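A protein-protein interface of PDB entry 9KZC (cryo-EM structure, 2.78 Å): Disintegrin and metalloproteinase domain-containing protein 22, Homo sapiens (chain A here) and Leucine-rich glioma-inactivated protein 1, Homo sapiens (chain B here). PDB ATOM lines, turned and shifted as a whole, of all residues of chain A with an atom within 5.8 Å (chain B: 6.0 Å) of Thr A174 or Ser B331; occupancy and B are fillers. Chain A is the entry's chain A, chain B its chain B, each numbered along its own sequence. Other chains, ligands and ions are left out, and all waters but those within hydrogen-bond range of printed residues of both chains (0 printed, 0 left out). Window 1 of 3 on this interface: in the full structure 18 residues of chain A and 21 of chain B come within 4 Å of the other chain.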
ATOM      1  N   LEU A 133     -19.114   9.503  26.703  1.00  0.00           N
ATOM      2  CA  LEU A 133     -20.373  10.239  26.772  1.00  0.00           C
ATOM      3  C   LEU A 133     -21.067  10.016  28.108  1.00  0.00           C
ATOM      4  O   LEU A 133     -21.585  10.961  28.719  1.00  0.00           O
ATOM      5  CB  LEU A 133     -21.287   9.823  25.621  1.00  0.00           C
ATOM      6  CG  LEU A 133     -22.773  10.143  25.794  1.00  0.00           C
ATOM      7  CD1 LEU A 133     -23.028  11.631  25.635  1.00  0.00           C
ATOM      8  CD2 LEU A 133     -23.616   9.345  24.817  1.00  0.00           C
ATOM      9  N   VAL A 136     -19.420  11.944  30.775  1.00  0.00           N
ATOM     10  CA  VAL A 136     -19.870  13.336  30.752  1.00  0.00           C
ATOM     11  C   VAL A 136     -21.238  13.466  31.417  1.00  0.00           C
ATOM     12  O   VAL A 136     -21.500  14.420  32.164  1.00  0.00           O
ATOM     13  CB  VAL A 136     -19.887  13.864  29.304  1.00  0.00           C
ATOM     14  CG1 VAL A 136     -20.658  15.173  29.211  1.00  0.00           C
ATOM     15  CG2 VAL A 136     -18.470  14.040  28.788  1.00  0.00           C
ATOM     16  N   GLN A 140     -22.119  15.734  34.740  1.00  0.00           N
ATOM     17  CA  GLN A 140     -23.122  16.790  34.862  1.00  0.00           C
ATOM     18  C   GLN A 140     -24.169  16.457  35.924  1.00  0.00           C
ATOM     19  O   GLN A 140     -24.656  17.363  36.613  1.00  0.00           O
ATOM     20  CB  GLN A 140     -23.769  17.077  33.505  1.00  0.00           C
ATOM     21  CG  GLN A 140     -24.596  15.963  32.914  1.00  0.00           C
ATOM     22  CD  GLN A 140     -25.116  16.303  31.531  1.00  0.00           C
ATOM     23  OE1 GLN A 140     -24.887  17.399  31.021  1.00  0.00           O
ATOM     24  NE2 GLN A 140     -25.823  15.362  30.916  1.00  0.00           N
ATOM     25  N   CYS A 169     -19.740  23.274  26.558  1.00  0.00           N
ATOM     26  CA  CYS A 169     -19.388  23.019  27.945  1.00  0.00           C
ATOM     27  C   CYS A 169     -20.278  21.917  28.502  1.00  0.00           C
ATOM     28  O   CYS A 169     -21.239  21.477  27.865  1.00  0.00           O
ATOM     29  CB  CYS A 169     -19.492  24.300  28.782  1.00  0.00           C
ATOM     30  SG  CYS A 169     -18.054  25.397  28.620  1.00  0.00           S
ATOM     31  N   ILE A 170     -19.939  21.466  29.710  1.00  0.00           N
ATOM     32  CA  ILE A 170     -20.542  20.251  30.252  1.00  0.00           C
ATOM     33  C   ILE A 170     -22.024  20.457  30.550  1.00  0.00           C
ATOM     34  O   ILE A 170     -22.841  19.551  30.350  1.00  0.00           O
ATOM     35  CB  ILE A 170     -19.764  19.786  31.496  1.00  0.00           C
ATOM     36  CG1 ILE A 170     -18.334  19.411  31.105  1.00  0.00           C
ATOM     37  CG2 ILE A 170     -20.453  18.608  32.159  1.00  0.00           C
ATOM     38  CD1 ILE A 170     -17.420  19.184  32.275  1.00  0.00           C
ATOM     39  N   GLY A 172     -24.229  22.241  29.039  1.00  0.00           N
ATOM     40  CA  GLY A 172     -25.076  22.364  27.874  1.00  0.00           C
ATOM     41  C   GLY A 172     -25.489  21.020  27.303  1.00  0.00           C
ATOM     42  O   GLY A 172     -25.067  19.955  27.751  1.00  0.00           O
ATOM     43  N   ASP A 173     -26.346  21.086  26.287  1.00  0.00           N
ATOM     44  CA  ASP A 173     -26.774  19.881  25.589  1.00  0.00           C
ATOM     45  C   ASP A 173     -25.604  19.263  24.835  1.00  0.00           C
ATOM     46  O   ASP A 173     -24.817  19.962  24.191  1.00  0.00           O
ATOM     47  CB  ASP A 173     -27.915  20.199  24.623  1.00  0.00           C
ATOM     48  CG  ASP A 173     -29.201  20.562  25.341  1.00  0.00           C
ATOM     49  OD1 ASP A 173     -29.412  20.069  26.469  1.00  0.00           O
ATOM     50  OD2 ASP A 173     -29.999  21.338  24.777  1.00  0.00           O
ATOM     51  N   THR A 174     -25.497  17.943  24.914  1.00  0.00           N
ATOM     52  CA  THR A 174     -24.339  17.215  24.415  1.00  0.00           C
ATOM     53  C   THR A 174     -24.616  16.658  23.025  1.00  0.00           C
ATOM     54  O   THR A 174     -25.654  16.028  22.798  1.00  0.00           O
ATOM     55  CB  THR A 174     -23.968  16.079  25.368  1.00  0.00           C
ATOM     56  OG1 THR A 174     -24.007  16.557  26.718  1.00  0.00           O
ATOM     57  CG2 THR A 174     -22.577  15.578  25.069  1.00  0.00           C
ATOM     58  N   GLY A 175     -23.686  16.894  22.103  1.00  0.00           N
ATOM     59  CA  GLY A 175     -23.763  16.322  20.774  1.00  0.00           C
ATOM     60  C   GLY A 175     -22.741  15.223  20.572  1.00  0.00           C
ATOM     61  O   GLY A 175     -22.346  14.557  21.533  1.00  0.00           O
ATOM     62  N   TYR A 176     -22.305  15.015  19.328  1.00  0.00           N
ATOM     63  CA  TYR A 176     -21.270  14.018  19.074  1.00  0.00           C
ATOM     64  C   TYR A 176     -19.938  14.440  19.682  1.00  0.00           C
ATOM     65  O   TYR A 176     -19.203  13.604  20.220  1.00  0.00           O
ATOM     66  CB  TYR A 176     -21.117  13.775  17.574  1.00  0.00           C
ATOM     67  CG  TYR A 176     -19.992  12.824  17.243  1.00  0.00           C
ATOM     68  CD1 TYR A 176     -20.074  11.481  17.582  1.00  0.00           C
ATOM     69  CD2 TYR A 176     -18.843  13.270  16.606  1.00  0.00           C
ATOM     70  CE1 TYR A 176     -19.047  10.608  17.291  1.00  0.00           C
ATOM     71  CE2 TYR A 176     -17.810  12.404  16.311  1.00  0.00           C
ATOM     72  CZ  TYR A 176     -17.918  11.074  16.655  1.00  0.00           C
ATOM     73  OH  TYR A 176     -16.892  10.207  16.363  1.00  0.00           O
ATOM     74  N   TYR A 177     -19.610  15.725  19.602  1.00  0.00           N
ATOM     75  CA  TYR A 177     -18.365  16.250  20.152  1.00  0.00           C
ATOM     76  C   TYR A 177     -18.591  16.588  21.619  1.00  0.00           C
ATOM     77  O   TYR A 177     -19.245  17.584  21.944  1.00  0.00           O
ATOM     78  CB  TYR A 177     -17.898  17.463  19.355  1.00  0.00           C
ATOM     79  CG  TYR A 177     -17.564  17.132  17.920  1.00  0.00           C
ATOM     80  CD1 TYR A 177     -16.375  16.493  17.598  1.00  0.00           C
ATOM     81  CD2 TYR A 177     -18.440  17.441  16.889  1.00  0.00           C
ATOM     82  CE1 TYR A 177     -16.062  16.180  16.293  1.00  0.00           C
ATOM     83  CE2 TYR A 177     -18.136  17.131  15.578  1.00  0.00           C
ATOM     84  CZ  TYR A 177     -16.946  16.500  15.287  1.00  0.00           C
ATOM     85  OH  TYR A 177     -16.636  16.189  13.984  1.00  0.00           O
ATOM     86  N   LEU A 178     -18.052  15.759  22.497  1.00  0.00           N
ATOM     87  CA  LEU A 178     -18.338  15.847  23.920  1.00  0.00           C
ATOM     88  C   LEU A 178     -17.583  17.009  24.557  1.00  0.00           C
ATOM     89  O   LEU A 178     -16.437  17.282  24.191  1.00  0.00           O
ATOM     90  CB  LEU A 178     -17.960  14.550  24.618  1.00  0.00           C
ATOM     91  CG  LEU A 178     -18.558  13.290  24.006  1.00  0.00           C
ATOM     92  CD1 LEU A 178     -17.983  12.104  24.709  1.00  0.00           C
ATOM     93  CD2 LEU A 178     -20.065  13.292  24.113  1.00  0.00           C
ATOM     94  N   PRO A 179     -18.199  17.698  25.511  1.00  0.00           N
ATOM     95  CA  PRO A 179     -17.495  18.764  26.227  1.00  0.00           C
ATOM     96  C   PRO A 179     -16.438  18.203  27.162  1.00  0.00           C
ATOM     97  O   PRO A 179     -16.429  17.019  27.507  1.00  0.00           O
ATOM     98  CB  PRO A 179     -18.610  19.463  27.009  1.00  0.00           C
ATOM     99  CG  PRO A 179     -19.675  18.434  27.145  1.00  0.00           C
ATOM    100  CD  PRO A 179     -19.613  17.603  25.907  1.00  0.00           C
ATOM    101  N   LEU B 282     -22.242  24.070  14.736  1.00  0.00           N
ATOM    102  CA  LEU B 282     -22.399  23.610  16.110  1.00  0.00           C
ATOM    103  C   LEU B 282     -22.722  24.764  17.048  1.00  0.00           C
ATOM    104  O   LEU B 282     -23.352  24.557  18.091  1.00  0.00           O
ATOM    105  CB  LEU B 282     -21.134  22.888  16.572  1.00  0.00           C
ATOM    106  CG  LEU B 282     -20.909  21.484  16.011  1.00  0.00           C
ATOM    107  CD1 LEU B 282     -19.706  20.833  16.665  1.00  0.00           C
ATOM    108  CD2 LEU B 282     -22.150  20.627  16.189  1.00  0.00           C
ATOM    109  N   LYS B 311     -27.278  20.108  17.353  1.00  0.00           N
ATOM    110  CA  LYS B 311     -25.936  19.556  17.177  1.00  0.00           C
ATOM    111  C   LYS B 311     -25.902  18.740  15.892  1.00  0.00           C
ATOM    112  O   LYS B 311     -25.862  17.505  15.924  1.00  0.00           O
ATOM    113  CB  LYS B 311     -25.532  18.702  18.379  1.00  0.00           C
ATOM    114  CG  LYS B 311     -25.419  19.473  19.680  1.00  0.00           C
ATOM    115  CD  LYS B 311     -24.330  20.524  19.599  1.00  0.00           C
ATOM    116  CE  LYS B 311     -24.018  21.104  20.964  1.00  0.00           C
ATOM    117  NZ  LYS B 311     -22.701  21.795  20.973  1.00  0.00           N
ATOM    118  N   PRO B 312     -25.920  19.405  14.737  1.00  0.00           N
ATOM    119  CA  PRO B 312     -25.891  18.670  13.469  1.00  0.00           C
ATOM    120  C   PRO B 312     -24.578  17.924  13.284  1.00  0.00           C
ATOM    121  O   PRO B 312     -23.518  18.358  13.740  1.00  0.00           O
ATOM    122  CB  PRO B 312     -26.060  19.772  12.417  1.00  0.00           C
ATOM    123  CG  PRO B 312     -25.581  21.007  13.085  1.00  0.00           C
ATOM    124  CD  PRO B 312     -25.937  20.863  14.530  1.00  0.00           C
ATOM    125  N   ASN B 313     -24.663  16.783  12.607  1.00  0.00           N
ATOM    126  CA  ASN B 313     -23.489  15.986  12.281  1.00  0.00           C
ATOM    127  C   ASN B 313     -23.389  15.611  10.813  1.00  0.00           C
ATOM    128  O   ASN B 313     -22.278  15.341  10.343  1.00  0.00           O
ATOM    129  CB  ASN B 313     -23.461  14.699  13.119  1.00  0.00           C
ATOM    130  CG  ASN B 313     -22.051  14.243  13.439  1.00  0.00           C
ATOM    131  OD1 ASN B 313     -21.202  15.041  13.828  1.00  0.00           O
ATOM    132  ND2 ASN B 313     -21.796  12.952  13.276  1.00  0.00           N
ATOM    133  N   ALA B 329     -28.779  15.252  10.303  1.00  0.00           N
ATOM    134  CA  ALA B 329     -28.629  14.300  11.395  1.00  0.00           C
ATOM    135  C   ALA B 329     -28.206  15.056  12.647  1.00  0.00           C
ATOM    136  O   ALA B 329     -27.124  15.651  12.683  1.00  0.00           O
ATOM    137  CB  ALA B 329     -27.609  13.221  11.040  1.00  0.00           C
ATOM    138  N   ASP B 330     -29.053  15.031  13.670  1.00  0.00           N
ATOM    139  CA  ASP B 330     -28.818  15.768  14.903  1.00  0.00           C
ATOM    140  C   ASP B 330     -28.314  14.804  15.969  1.00  0.00           C
ATOM    141  O   ASP B 330     -29.009  13.848  16.327  1.00  0.00           O
ATOM    142  CB  ASP B 330     -30.094  16.472  15.360  1.00  0.00           C
ATOM    143  CG  ASP B 330     -29.815  17.692  16.212  1.00  0.00           C
ATOM    144  OD1 ASP B 330     -28.800  17.699  16.935  1.00  0.00           O
ATOM    145  OD2 ASP B 330     -30.609  18.651  16.148  1.00  0.00           O
ATOM    146  N   SER B 331     -27.113  15.066  16.479  1.00  0.00           N
ATOM    147  CA  SER B 331     -26.441  14.177  17.416  1.00  0.00           C
ATOM    148  C   SER B 331     -26.802  14.457  18.869  1.00  0.00           C
ATOM    149  O   SER B 331     -26.165  13.902  19.769  1.00  0.00           O
ATOM    150  CB  SER B 331     -24.925  14.273  17.228  1.00  0.00           C
ATOM    151  OG  SER B 331     -24.517  15.619  17.074  1.00  0.00           O
ATOM    152  N   SER B 332     -27.799  15.297  19.118  1.00  0.00           N
ATOM    153  CA  SER B 332     -28.261  15.595  20.462  1.00  0.00           C
ATOM    154  C   SER B 332     -29.603  14.919  20.714  1.00  0.00           C
ATOM    155  O   SER B 332     -30.368  14.656  19.783  1.00  0.00           O
ATOM    156  CB  SER B 332     -28.390  17.105  20.677  1.00  0.00           C
ATOM    157  OG  SER B 332     -29.184  17.695  19.663  1.00  0.00           O
ATOM    158  N   LYS B 333     -29.873  14.622  21.987  1.00  0.00           N
ATOM    159  CA  LYS B 333     -31.166  14.053  22.350  1.00  0.00           C
ATOM    160  C   LYS B 333     -32.293  15.052  22.122  1.00  0.00           C
ATOM    161  O   LYS B 333     -33.370  14.682  21.640  1.00  0.00           O
ATOM    162  CB  LYS B 333     -31.149  13.594  23.806  1.00  0.00           C
ATOM    163  CG  LYS B 333     -30.304  12.363  24.064  1.00  0.00           C
ATOM    164  CD  LYS B 333     -30.750  11.658  25.330  1.00  0.00           C
ATOM    165  CE  LYS B 333     -32.140  11.074  25.166  1.00  0.00           C
ATOM    166  NZ  LYS B 333     -32.644  10.475  26.428  1.00  0.00           N
ATOM    167  N   GLY B 335     -32.452  17.616  19.983  1.00  0.00           N
ATOM    168  CA  GLY B 335     -32.685  17.867  18.572  1.00  0.00           C
ATOM    169  C   GLY B 335     -32.961  16.579  17.814  1.00  0.00           C
ATOM    170  O   GLY B 335     -32.288  15.570  18.008  1.00  0.00           O
ATOM    171  N   TYR B 357     -32.706  10.361  20.016  1.00  0.00           N
ATOM    172  CA  TYR B 357     -31.527   9.601  19.639  1.00  0.00           C
ATOM    173  C   TYR B 357     -30.426  10.541  19.170  1.00  0.00           C
ATOM    174  O   TYR B 357     -30.693  11.627  18.649  1.00  0.00           O
ATOM    175  CB  TYR B 357     -31.851   8.589  18.537  1.00  0.00           C
ATOM    176  CG  TYR B 357     -32.560   7.349  19.027  1.00  0.00           C
ATOM    177  CD1 TYR B 357     -33.939   7.325  19.165  1.00  0.00           C
ATOM    178  CD2 TYR B 357     -31.853   6.199  19.339  1.00  0.00           C
ATOM    179  CE1 TYR B 357     -34.594   6.197  19.605  1.00  0.00           C
ATOM    180  CE2 TYR B 357     -32.500   5.063  19.780  1.00  0.00           C
ATOM    181  CZ  TYR B 357     -33.870   5.068  19.913  1.00  0.00           C
ATOM    182  OH  TYR B 357     -34.519   3.939  20.352  1.00  0.00           O
ATOM    183  N   ARG B 358     -29.180  10.112  19.366  1.00  0.00           N
ATOM    184  CA  ARG B 358     -28.011  10.897  18.977  1.00  0.00           C
ATOM    185  C   ARG B 358     -27.538  10.410  17.611  1.00  0.00           C
ATOM    186  O   ARG B 358     -26.598   9.626  17.486  1.00  0.00           O
ATOM    187  CB  ARG B 358     -26.920  10.783  20.033  1.00  0.00           C
ATOM    188  CG  ARG B 358     -27.389  11.094  21.443  1.00  0.00           C
ATOM    189  CD  ARG B 358     -26.288  10.831  22.453  1.00  0.00           C
ATOM    190  NE  ARG B 358     -26.665  11.254  23.795  1.00  0.00           N
ATOM    191  CZ  ARG B 358     -26.459  12.469  24.284  1.00  0.00           C
ATOM    192  NH1 ARG B 358     -25.889  13.417  23.559  1.00  0.00           N
ATOM    193  NH2 ARG B 358     -26.833  12.739  25.530  1.00  0.00           N
ATOM    194  N   ASP B 359     -28.206  10.899  16.569  1.00  0.00           N
ATOM    195  CA  ASP B 359     -27.902  10.466  15.212  1.00  0.00           C
ATOM    196  C   ASP B 359     -26.592  11.078  14.735  1.00  0.00           C
ATOM    197  O   ASP B 359     -26.378  12.288  14.850  1.00  0.00           O
ATOM    198  CB  ASP B 359     -29.040  10.850  14.269  1.00  0.00           C
ATOM    199  CG  ASP B 359     -30.356  10.212  14.657  1.00  0.00           C
ATOM    200  OD1 ASP B 359     -30.396   8.974  14.808  1.00  0.00           O
ATOM    201  OD2 ASP B 359     -31.351  10.949  14.812  1.00  0.00           O
ATOM    202  N   THR B 360     -25.713  10.237  14.188  1.00  0.00           N
ATOM    203  CA  THR B 360     -24.420  10.687  13.697  1.00  0.00           C
ATOM    204  C   THR B 360     -24.315  10.710  12.180  1.00  0.00           C
ATOM    205  O   THR B 360     -23.430  11.390  11.651  1.00  0.00           O
ATOM    206  CB  THR B 360     -23.296   9.802  14.253  1.00  0.00           C
ATOM    207  OG1 THR B 360     -23.554   8.432  13.924  1.00  0.00           O
ATOM    208  CG2 THR B 360     -23.204   9.945  15.762  1.00  0.00           C
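The backbone carbonyl oxygen (O) of Asp B359 sits close to the backbone NH (N) of Ser B331 (3.3 Å).
N of Asn B313 is in hydrogen-bond range of O of Ala B329, at 2.7 Å.
The side-chain hydroxyl (OG) of Ser B332 lies within hydrogen-bond range of the backbone NH (N) of Gly B335.
The side-chain hydroxyl (OG) of Ser B331 lies within hydrogen-bond range of the backbone carbonyl oxygen (O) of Lys B311, at 2.6 Å.
The side-chain amide nitrogen of Asn B313 is in hydrogen-bond range of the backbone carbonyl oxygen of Thr B360 (2.8 Å).
The side-chain carboxylate (OD1) of Asp B330 lies within hydrogen-bond range of the backbone NH (N) of Lys B311 (2.9 Å).
Leu A133 touches Arg B358.
Lys B311 touches Asp A173 (CE to O, 3.5 Å).
Ser B331 touches Thr A174 (O to O, 3.7 Å).
Thr A174 touches Ser B332.
Gly A175 touches Lys B311 (CA to CG, 3.7 Å).
CA of Gly A175 touches O of Ser B331, at 3.6 Å.
Tyr A176 touches Asn B313 (CB to OD1, 3.96 Å).
Thr B360 touches Tyr A176.
Tyr A177 touches Leu B282.
Printed residues of chain B within 4 Å of Leu A133: Arg B358 (3.7 Å).
Gly A172 touches none of the printed residues of chain B.
Of chain B, only Ser B331, Ser B332 and Arg B358 come within 4 Å of Thr A174.
Leu A178 touches none of the printed residues of chain B.
Ser B331 touches just these residues of chain A: Thr A174, Gly A175 and Tyr A176.
Of the printed residues of chain A, Ser B332 touches Thr A174 (3.5 Å).
Of the printed residues of chain A, Arg B358 touches Leu A133 (3.7 Å) and Thr A174 (2.7 Å).
The nearest residue of chain B that does not touch Thr A174 is Lys B311 (4.4 Å).
Of the 13 printed residues of chain A, 6 touch a printed residue of chain B.
Printed residues of chain A that touch a printed residue of chain B: Leu A133, Asp A173, Thr A174, Gly A175, Tyr A176 and Tyr A177.
Hydrophobic or aromatic side chains of chain A within 4 Å of the printed part of chain B: Leu A133, Tyr A176 and Tyr A177.
Of the 14 printed residues of chain B, 7 touch a printed residue of chain A.
Printed residues of chain B that touch a printed residue of chain A: Leu B282, Lys B311, Asn B313, Ser B331, Ser B332, Arg B358 and Thr B360.
N of Tyr A176 is in hydrogen-bond range of OG of Ser B331 (3.2 Å).
NH1 of Arg B358 is in hydrogen-bond range of O of Thr A174 (2.7 Å).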
